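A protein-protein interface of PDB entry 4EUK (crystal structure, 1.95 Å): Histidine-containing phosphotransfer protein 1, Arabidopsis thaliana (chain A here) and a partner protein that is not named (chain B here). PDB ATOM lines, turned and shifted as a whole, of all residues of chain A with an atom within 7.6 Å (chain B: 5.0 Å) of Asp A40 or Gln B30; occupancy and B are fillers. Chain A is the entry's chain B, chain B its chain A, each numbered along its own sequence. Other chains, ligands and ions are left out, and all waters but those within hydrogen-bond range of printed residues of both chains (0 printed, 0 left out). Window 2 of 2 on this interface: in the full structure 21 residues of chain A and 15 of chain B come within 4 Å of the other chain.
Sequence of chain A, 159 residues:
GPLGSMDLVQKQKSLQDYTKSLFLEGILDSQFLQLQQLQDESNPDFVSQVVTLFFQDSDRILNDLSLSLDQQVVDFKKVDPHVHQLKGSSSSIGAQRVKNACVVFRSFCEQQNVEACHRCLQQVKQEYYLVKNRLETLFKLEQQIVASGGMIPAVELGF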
ATOM      1  N   GLN A  34       2.347  -3.385 -18.854  1.00  0.00           N
ATOM      2  CA  GLN A  34       3.585  -2.869 -19.473  1.00  0.00           C
ATOM      3  C   GLN A  34       4.055  -1.657 -18.728  1.00  0.00           C
ATOM      4  O   GLN A  34       5.235  -1.519 -18.454  1.00  0.00           O
ATOM      5  CB  GLN A  34       3.377  -2.434 -20.935  1.00  0.00           C
ATOM      6  CG  GLN A  34       3.155  -3.517 -21.881  1.00  0.00           C
ATOM      7  CD  GLN A  34       4.415  -4.284 -22.238  1.00  0.00           C
ATOM      8  OE1 GLN A  34       5.483  -3.704 -22.483  1.00  0.00           O
ATOM      9  NE2 GLN A  34       4.283  -5.605 -22.302  1.00  0.00           N
ATOM     10  N   LEU A  35       3.127  -0.757 -18.390  1.00  0.00           N
ATOM     11  CA  LEU A  35       3.511   0.451 -17.673  1.00  0.00           C
ATOM     12  C   LEU A  35       4.056   0.101 -16.288  1.00  0.00           C
ATOM     13  O   LEU A  35       5.069   0.663 -15.850  1.00  0.00           O
ATOM     14  CB  LEU A  35       2.335   1.425 -17.520  1.00  0.00           C
ATOM     15  CG  LEU A  35       1.552   1.834 -18.762  1.00  0.00           C
ATOM     16  CD1 LEU A  35       0.494   2.880 -18.403  1.00  0.00           C
ATOM     17  CD2 LEU A  35       2.488   2.377 -19.823  1.00  0.00           C
ATOM     18  N   GLN A  36       3.383  -0.808 -15.590  1.00  0.00           N
ATOM     19  CA  GLN A  36       3.838  -1.201 -14.250  1.00  0.00           C
ATOM     20  C   GLN A  36       5.221  -1.841 -14.303  1.00  0.00           C
ATOM     21  O   GLN A  36       6.045  -1.607 -13.426  1.00  0.00           O
ATOM     22  CB  GLN A  36       2.839  -2.150 -13.595  1.00  0.00           C
ATOM     23  CG  GLN A  36       1.543  -1.469 -13.202  1.00  0.00           C
ATOM     24  CD  GLN A  36       0.599  -2.401 -12.436  1.00  0.00           C
ATOM     25  OE1 GLN A  36       0.299  -3.500 -12.898  1.00  0.00           O
ATOM     26  NE2 GLN A  36       0.099  -1.944 -11.297  1.00  0.00           N
ATOM     27  N   GLN A  37       5.483  -2.626 -15.345  1.00  0.00           N
ATOM     28  CA  GLN A  37       6.801  -3.242 -15.544  1.00  0.00           C
ATOM     29  C   GLN A  37       7.921  -2.211 -15.722  1.00  0.00           C
ATOM     30  O   GLN A  37       9.051  -2.473 -15.345  1.00  0.00           O
ATOM     31  CB  GLN A  37       6.815  -4.173 -16.784  1.00  0.00           C
ATOM     32  CG  GLN A  37       6.051  -5.496 -16.670  1.00  0.00           C
ATOM     33  CD  GLN A  37       5.830  -6.178 -18.046  1.00  0.00           C
ATOM     34  OE1 GLN A  37       4.745  -6.700 -18.326  1.00  0.00           O
ATOM     35  NE2 GLN A  37       6.862  -6.154 -18.906  1.00  0.00           N
ATOM     36  N   LEU A  38       7.608  -1.054 -16.294  1.00  0.00           N
ATOM     37  CA  LEU A  38       8.599   0.008 -16.520  1.00  0.00           C
ATOM     38  C   LEU A  38       8.951   0.808 -15.251  1.00  0.00           C
ATOM     39  O   LEU A  38       9.986   1.478 -15.183  1.00  0.00           O
ATOM     40  CB  LEU A  38       8.094   0.962 -17.606  1.00  0.00           C
ATOM     41  CG  LEU A  38       8.001   0.367 -19.020  1.00  0.00           C
ATOM     42  CD1 LEU A  38       7.210   1.273 -19.932  1.00  0.00           C
ATOM     43  CD2 LEU A  38       9.409   0.102 -19.629  1.00  0.00           C
ATOM     44  N   GLN A  39       8.090   0.732 -14.250  1.00  0.00           N
ATOM     45  CA  GLN A  39       8.314   1.439 -12.991  1.00  0.00           C
ATOM     46  C   GLN A  39       9.248   0.642 -12.086  1.00  0.00           C
ATOM     47  O   GLN A  39       8.922  -0.472 -11.683  1.00  0.00           O
ATOM     48  CB  GLN A  39       6.985   1.666 -12.302  1.00  0.00           C
ATOM     49  CG  GLN A  39       7.038   2.475 -11.009  1.00  0.00           C
ATOM     50  CD  GLN A  39       5.664   2.933 -10.596  1.00  0.00           C
ATOM     51  OE1 GLN A  39       5.154   3.950 -11.081  1.00  0.00           O
ATOM     52  NE2 GLN A  39       5.042   2.181  -9.716  1.00  0.00           N
ATOM     53  N   ASP A  40      10.398   1.229 -11.765  1.00  0.00           N
ATOM     54  CA  ASP A  40      11.405   0.594 -10.894  1.00  0.00           C
ATOM     55  C   ASP A  40      12.221   1.685 -10.189  1.00  0.00           C
ATOM     56  O   ASP A  40      11.863   2.863 -10.279  1.00  0.00           O
ATOM     57  CB  ASP A  40      12.308  -0.369 -11.695  1.00  0.00           C
ATOM     58  CG  ASP A  40      13.011   0.301 -12.891  1.00  0.00           C
ATOM     59  OD1 ASP A  40      13.177   1.543 -12.908  1.00  0.00           O
ATOM     60  OD2 ASP A  40      13.404  -0.434 -13.832  1.00  0.00           O
ATOM     61  N   GLU A  41      13.302   1.304  -9.494  1.00  0.00           N
ATOM     62  CA  GLU A  41      14.184   2.272  -8.823  1.00  0.00           C
ATOM     63  C   GLU A  41      14.711   3.329  -9.810  1.00  0.00           C
ATOM     64  O   GLU A  41      14.827   4.500  -9.467  1.00  0.00           O
ATOM     65  CB  GLU A  41      15.345   1.550  -8.119  1.00  0.00           C
ATOM     66  N   SER A  42      14.987   2.925 -11.043  1.00  0.00           N
ATOM     67  CA  SER A  42      15.377   3.864 -12.102  1.00  0.00           C
ATOM     68  C   SER A  42      14.246   4.786 -12.645  1.00  0.00           C
ATOM     69  O   SER A  42      14.538   5.714 -13.404  1.00  0.00           O
ATOM     70  CB  SER A  42      15.989   3.085 -13.271  1.00  0.00           C
ATOM     71  N   ASN A  43      12.981   4.542 -12.264  1.00  0.00           N
ATOM     72  CA  ASN A  43      11.820   5.281 -12.818  1.00  0.00           C
ATOM     73  C   ASN A  43      10.607   5.219 -11.831  1.00  0.00           C
ATOM     74  O   ASN A  43       9.552   4.669 -12.160  1.00  0.00           O
ATOM     75  CB  ASN A  43      11.480   4.669 -14.209  1.00  0.00           C
ATOM     76  CG  ASN A  43      10.986   5.702 -15.255  1.00  0.00           C
ATOM     77  OD1 ASN A  43      10.761   5.352 -16.424  1.00  0.00           O
ATOM     78  ND2 ASN A  43      10.810   6.952 -14.843  1.00  0.00           N
ATOM     79  N   PRO A  44      10.745   5.795 -10.614  1.00  0.00           N
ATOM     80  CA  PRO A  44       9.918   5.409  -9.430  1.00  0.00           C
ATOM     81  C   PRO A  44       8.406   5.737  -9.395  1.00  0.00           C
ATOM     82  O   PRO A  44       7.616   5.018  -8.751  1.00  0.00           O
ATOM     83  CB  PRO A  44      10.634   6.115  -8.264  1.00  0.00           C
ATOM     84  CG  PRO A  44      11.984   6.438  -8.791  1.00  0.00           C
ATOM     85  CD  PRO A  44      11.805   6.743 -10.231  1.00  0.00           C
ATOM     86  N   ASP A  45       8.015   6.802 -10.079  1.00  0.00           N
ATOM     87  CA  ASP A  45       6.619   7.270 -10.137  1.00  0.00           C
ATOM     88  C   ASP A  45       6.101   7.235 -11.591  1.00  0.00           C
ATOM     89  O   ASP A  45       5.150   7.942 -11.949  1.00  0.00           O
ATOM     90  CB  ASP A  45       6.562   8.720  -9.645  1.00  0.00           C
ATOM     91  CG  ASP A  45       5.343   9.009  -8.804  1.00  0.00           C
ATOM     92  OD1 ASP A  45       4.336   8.281  -8.938  1.00  0.00           O
ATOM     93  OD2 ASP A  45       5.410   9.959  -7.974  1.00  0.00           O
ATOM     94  N   PHE A  46       6.729   6.411 -12.420  1.00  0.00           N
ATOM     95  CA  PHE A  46       6.398   6.365 -13.851  1.00  0.00           C
ATOM     96  C   PHE A  46       4.901   6.152 -14.163  1.00  0.00           C
ATOM     97  O   PHE A  46       4.333   6.896 -14.952  1.00  0.00           O
ATOM     98  CB  PHE A  46       7.245   5.328 -14.571  1.00  0.00           C
ATOM     99  CG  PHE A  46       6.881   5.176 -15.999  1.00  0.00           C
ATOM    100  CD1 PHE A  46       7.270   6.122 -16.917  1.00  0.00           C
ATOM    101  CD2 PHE A  46       6.083   4.115 -16.412  1.00  0.00           C
ATOM    102  CE1 PHE A  46       6.897   6.000 -18.257  1.00  0.00           C
ATOM    103  CE2 PHE A  46       5.715   3.988 -17.748  1.00  0.00           C
ATOM    104  CZ  PHE A  46       6.110   4.929 -18.662  1.00  0.00           C
ATOM    105  N   VAL A  47       4.251   5.154 -13.561  1.00  0.00           N
ATOM    106  CA  VAL A  47       2.831   4.902 -13.874  1.00  0.00           C
ATOM    107  C   VAL A  47       1.941   6.110 -13.580  1.00  0.00           C
ATOM    108  O   VAL A  47       1.144   6.527 -14.407  1.00  0.00           O
ATOM    109  CB  VAL A  47       2.286   3.660 -13.147  1.00  0.00           C
ATOM    110  CG1 VAL A  47       0.846   3.398 -13.563  1.00  0.00           C
ATOM    111  CG2 VAL A  47       3.142   2.460 -13.502  1.00  0.00           C
ATOM    112  N   ALA A 154       7.332  -5.125  -6.862  1.00  0.00           N
ATOM    113  CA  ALA A 154       7.477  -4.738  -8.261  1.00  0.00           C
ATOM    114  C   ALA A 154       6.853  -5.801  -9.133  1.00  0.00           C
ATOM    115  O   ALA A 154       6.975  -6.995  -8.856  1.00  0.00           O
ATOM    116  CB  ALA A 154       8.954  -4.550  -8.630  1.00  0.00           C
ATOM    117  N   SER B  26      10.380   5.506 -22.320  1.00  0.00           N
ATOM    118  CA  SER B  26      10.732   4.662 -21.183  1.00  0.00           C
ATOM    119  C   SER B  26      11.018   3.225 -21.606  1.00  0.00           C
ATOM    120  O   SER B  26      11.908   2.590 -21.070  1.00  0.00           O
ATOM    121  CB  SER B  26       9.644   4.708 -20.105  1.00  0.00           C
ATOM    122  OG  SER B  26       9.709   5.939 -19.416  1.00  0.00           O
ATOM    123  N   MET B  27      10.290   2.705 -22.585  1.00  0.00           N
ATOM    124  CA  MET B  27      10.572   1.358 -23.037  1.00  0.00           C
ATOM    125  C   MET B  27      11.963   1.303 -23.673  1.00  0.00           C
ATOM    126  O   MET B  27      12.749   0.373 -23.421  1.00  0.00           O
ATOM    127  CB  MET B  27       9.527   0.898 -24.031  1.00  0.00           C
ATOM    128  CG  MET B  27       8.171   0.621 -23.372  1.00  0.00           C
ATOM    129  SD  MET B  27       6.934   0.152 -24.612  1.00  0.00           S
ATOM    130  CE  MET B  27       5.581  -0.276 -23.482  1.00  0.00           C
ATOM    131  N   MET B  28      12.260   2.290 -24.513  1.00  0.00           N
ATOM    132  CA  MET B  28      13.537   2.314 -25.214  1.00  0.00           C
ATOM    133  C   MET B  28      14.672   2.513 -24.230  1.00  0.00           C
ATOM    134  O   MET B  28      15.750   1.954 -24.412  1.00  0.00           O
ATOM    135  CB  MET B  28      13.544   3.390 -26.313  1.00  0.00           C
ATOM    136  CG  MET B  28      12.737   2.958 -27.506  1.00  0.00           C
ATOM    137  SD  MET B  28      13.484   1.527 -28.367  1.00  0.00           S
ATOM    138  CE  MET B  28      15.043   2.276 -28.770  1.00  0.00           C
ATOM    139  N   LYS B  29      14.429   3.298 -23.180  1.00  0.00           N
ATOM    140  CA  LYS B  29      15.433   3.488 -22.138  1.00  0.00           C
ATOM    141  C   LYS B  29      15.733   2.183 -21.434  1.00  0.00           C
ATOM    142  O   LYS B  29      16.888   1.865 -21.183  1.00  0.00           O
ATOM    143  CB  LYS B  29      14.981   4.529 -21.115  1.00  0.00           C
ATOM    144  CG  LYS B  29      15.430   5.930 -21.448  1.00  0.00           C
ATOM    145  CD  LYS B  29      16.794   6.240 -20.821  1.00  0.00           C
ATOM    146  CE  LYS B  29      17.125   7.723 -20.919  1.00  0.00           C
ATOM    147  NZ  LYS B  29      18.241   8.077 -20.006  1.00  0.00           N
ATOM    148  N   GLN B  30      14.704   1.405 -21.133  1.00  0.00           N
ATOM    149  CA  GLN B  30      14.936   0.132 -20.453  1.00  0.00           C
ATOM    150  C   GLN B  30      15.713  -0.823 -21.355  1.00  0.00           C
ATOM    151  O   GLN B  30      16.460  -1.668 -20.877  1.00  0.00           O
ATOM    152  CB  GLN B  30      13.619  -0.496 -19.976  1.00  0.00           C
ATOM    153  CG  GLN B  30      13.726  -1.089 -18.588  1.00  0.00           C
ATOM    154  CD  GLN B  30      12.548  -1.966 -18.255  1.00  0.00           C
ATOM    155  OE1 GLN B  30      12.288  -2.948 -18.944  1.00  0.00           O
ATOM    156  NE2 GLN B  30      11.829  -1.621 -17.188  1.00  0.00           N
ATOM    157  N   LEU B  31      15.550  -0.672 -22.665  1.00  0.00           N
ATOM    158  CA  LEU B  31      16.312  -1.440 -23.645  1.00  0.00           C
ATOM    159  C   LEU B  31      17.710  -0.854 -23.910  1.00  0.00           C
ATOM    160  O   LEU B  31      18.471  -1.426 -24.668  1.00  0.00           O
ATOM    161  CB  LEU B  31      15.520  -1.550 -24.962  1.00  0.00           C
ATOM    162  CG  LEU B  31      14.571  -2.740 -25.220  1.00  0.00           C
ATOM    163  CD1 LEU B  31      14.023  -3.405 -23.990  1.00  0.00           C
ATOM    164  CD2 LEU B  31      13.456  -2.356 -26.198  1.00  0.00           C
ATOM    165  N   GLY B  32      18.044   0.281 -23.304  1.00  0.00           N
ATOM    166  CA  GLY B  32      19.402   0.812 -23.352  1.00  0.00           C
ATOM    167  C   GLY B  32      19.610   1.902 -24.389  1.00  0.00           C
ATOM    168  O   GLY B  32      20.747   2.201 -24.762  1.00  0.00           O
ATOM    169  N   LEU B 141       7.311  -3.606 -24.861  1.00  0.00           N
ATOM    170  CA  LEU B 141       8.737  -3.908 -24.775  1.00  0.00           C
ATOM    171  C   LEU B 141       9.134  -5.031 -25.710  1.00  0.00           C
ATOM    172  O   LEU B 141      10.140  -4.932 -26.392  1.00  0.00           O
ATOM    173  CB  LEU B 141       9.136  -4.318 -23.361  1.00  0.00           C
ATOM    174  CG  LEU B 141       9.737  -3.230 -22.502  1.00  0.00           C
ATOM    175  CD1 LEU B 141       9.839  -3.726 -21.056  1.00  0.00           C
ATOM    176  CD2 LEU B 141      11.113  -2.855 -23.073  1.00  0.00           C
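Gln A34 touches Met B27 (OE1 to CE, 3.6 Å).
CD2 of Leu A38 touches O of Ser B26, at 3.8 Å.
Leu A38 touches Met B27 (CD1 to CG, 3.6 Å).
Leu A38 touches Gln B30.
Asp A40 touches Gln B30 (OD2 to NE2, 3.9 Å).
Ser B26 touches Phe A46.
Of the printed residues of chain B, Asp A40 touches Gln B30 (3.9 Å).
Printed residues of chain B within 4 Å of Asn A43: Ser B26.
Of the printed residues of chain A, Met B27 touches Gln A34 (3.6 Å) and Leu A38 (3.6 Å).
Gln B30 touches just these residues of chain A: Gln A37 (3.4 Å), Leu A38 (3.7 Å) and Asp A40 (3.9 Å).
The nearest printed residue of chain B that does not touch Asp A40 is Ser B26 (8.0 Å).
The nearest printed residue of chain B that does not touch Gln A34 is Gln B30 (6.7 Å).
The side-chain carboxylate (OD1) of Asp A40 is in hydrogen-bond range of the backbone NH (N) of Asn A43 (3.1 Å).
The side-chain carboxylate (OD1) of Asp A40 sits at hydrogen-bond distance from the backbone NH (N) of Ser A42, 2.9 Å away.
OE1 of Gln A39 lies within hydrogen-bond range of N of Phe A46 (3.2 Å).
The backbone NH (N) of Leu B141 sits at hydrogen-bond distance from the side-chain sulfur (SD) of Met B27 (3.8 Å).
The backbone NH (N) of Leu B141 is in hydrogen-bond range of the side-chain amide oxygen (OE1) of Gln A34.
The side-chain amide nitrogen of Gln B30 lies within hydrogen-bond range of the backbone carbonyl oxygen of Gln A37 (3.4 Å).
The side-chain hydroxyl of Ser B26 sits at hydrogen-bond distance from the side-chain amide oxygen of Asn A43 (3.2 Å).
Printed residues of chain A that touch a printed residue of chain B: Gln A34, Gln A37, Leu A38, Asp A40, Asn A43 and Phe A46.
Hydrophobic or aromatic side chains of chain B that line the printed part of chain A: Met B27 and Leu B141.
Among the printed residues, 9 pairs touch across the chains.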
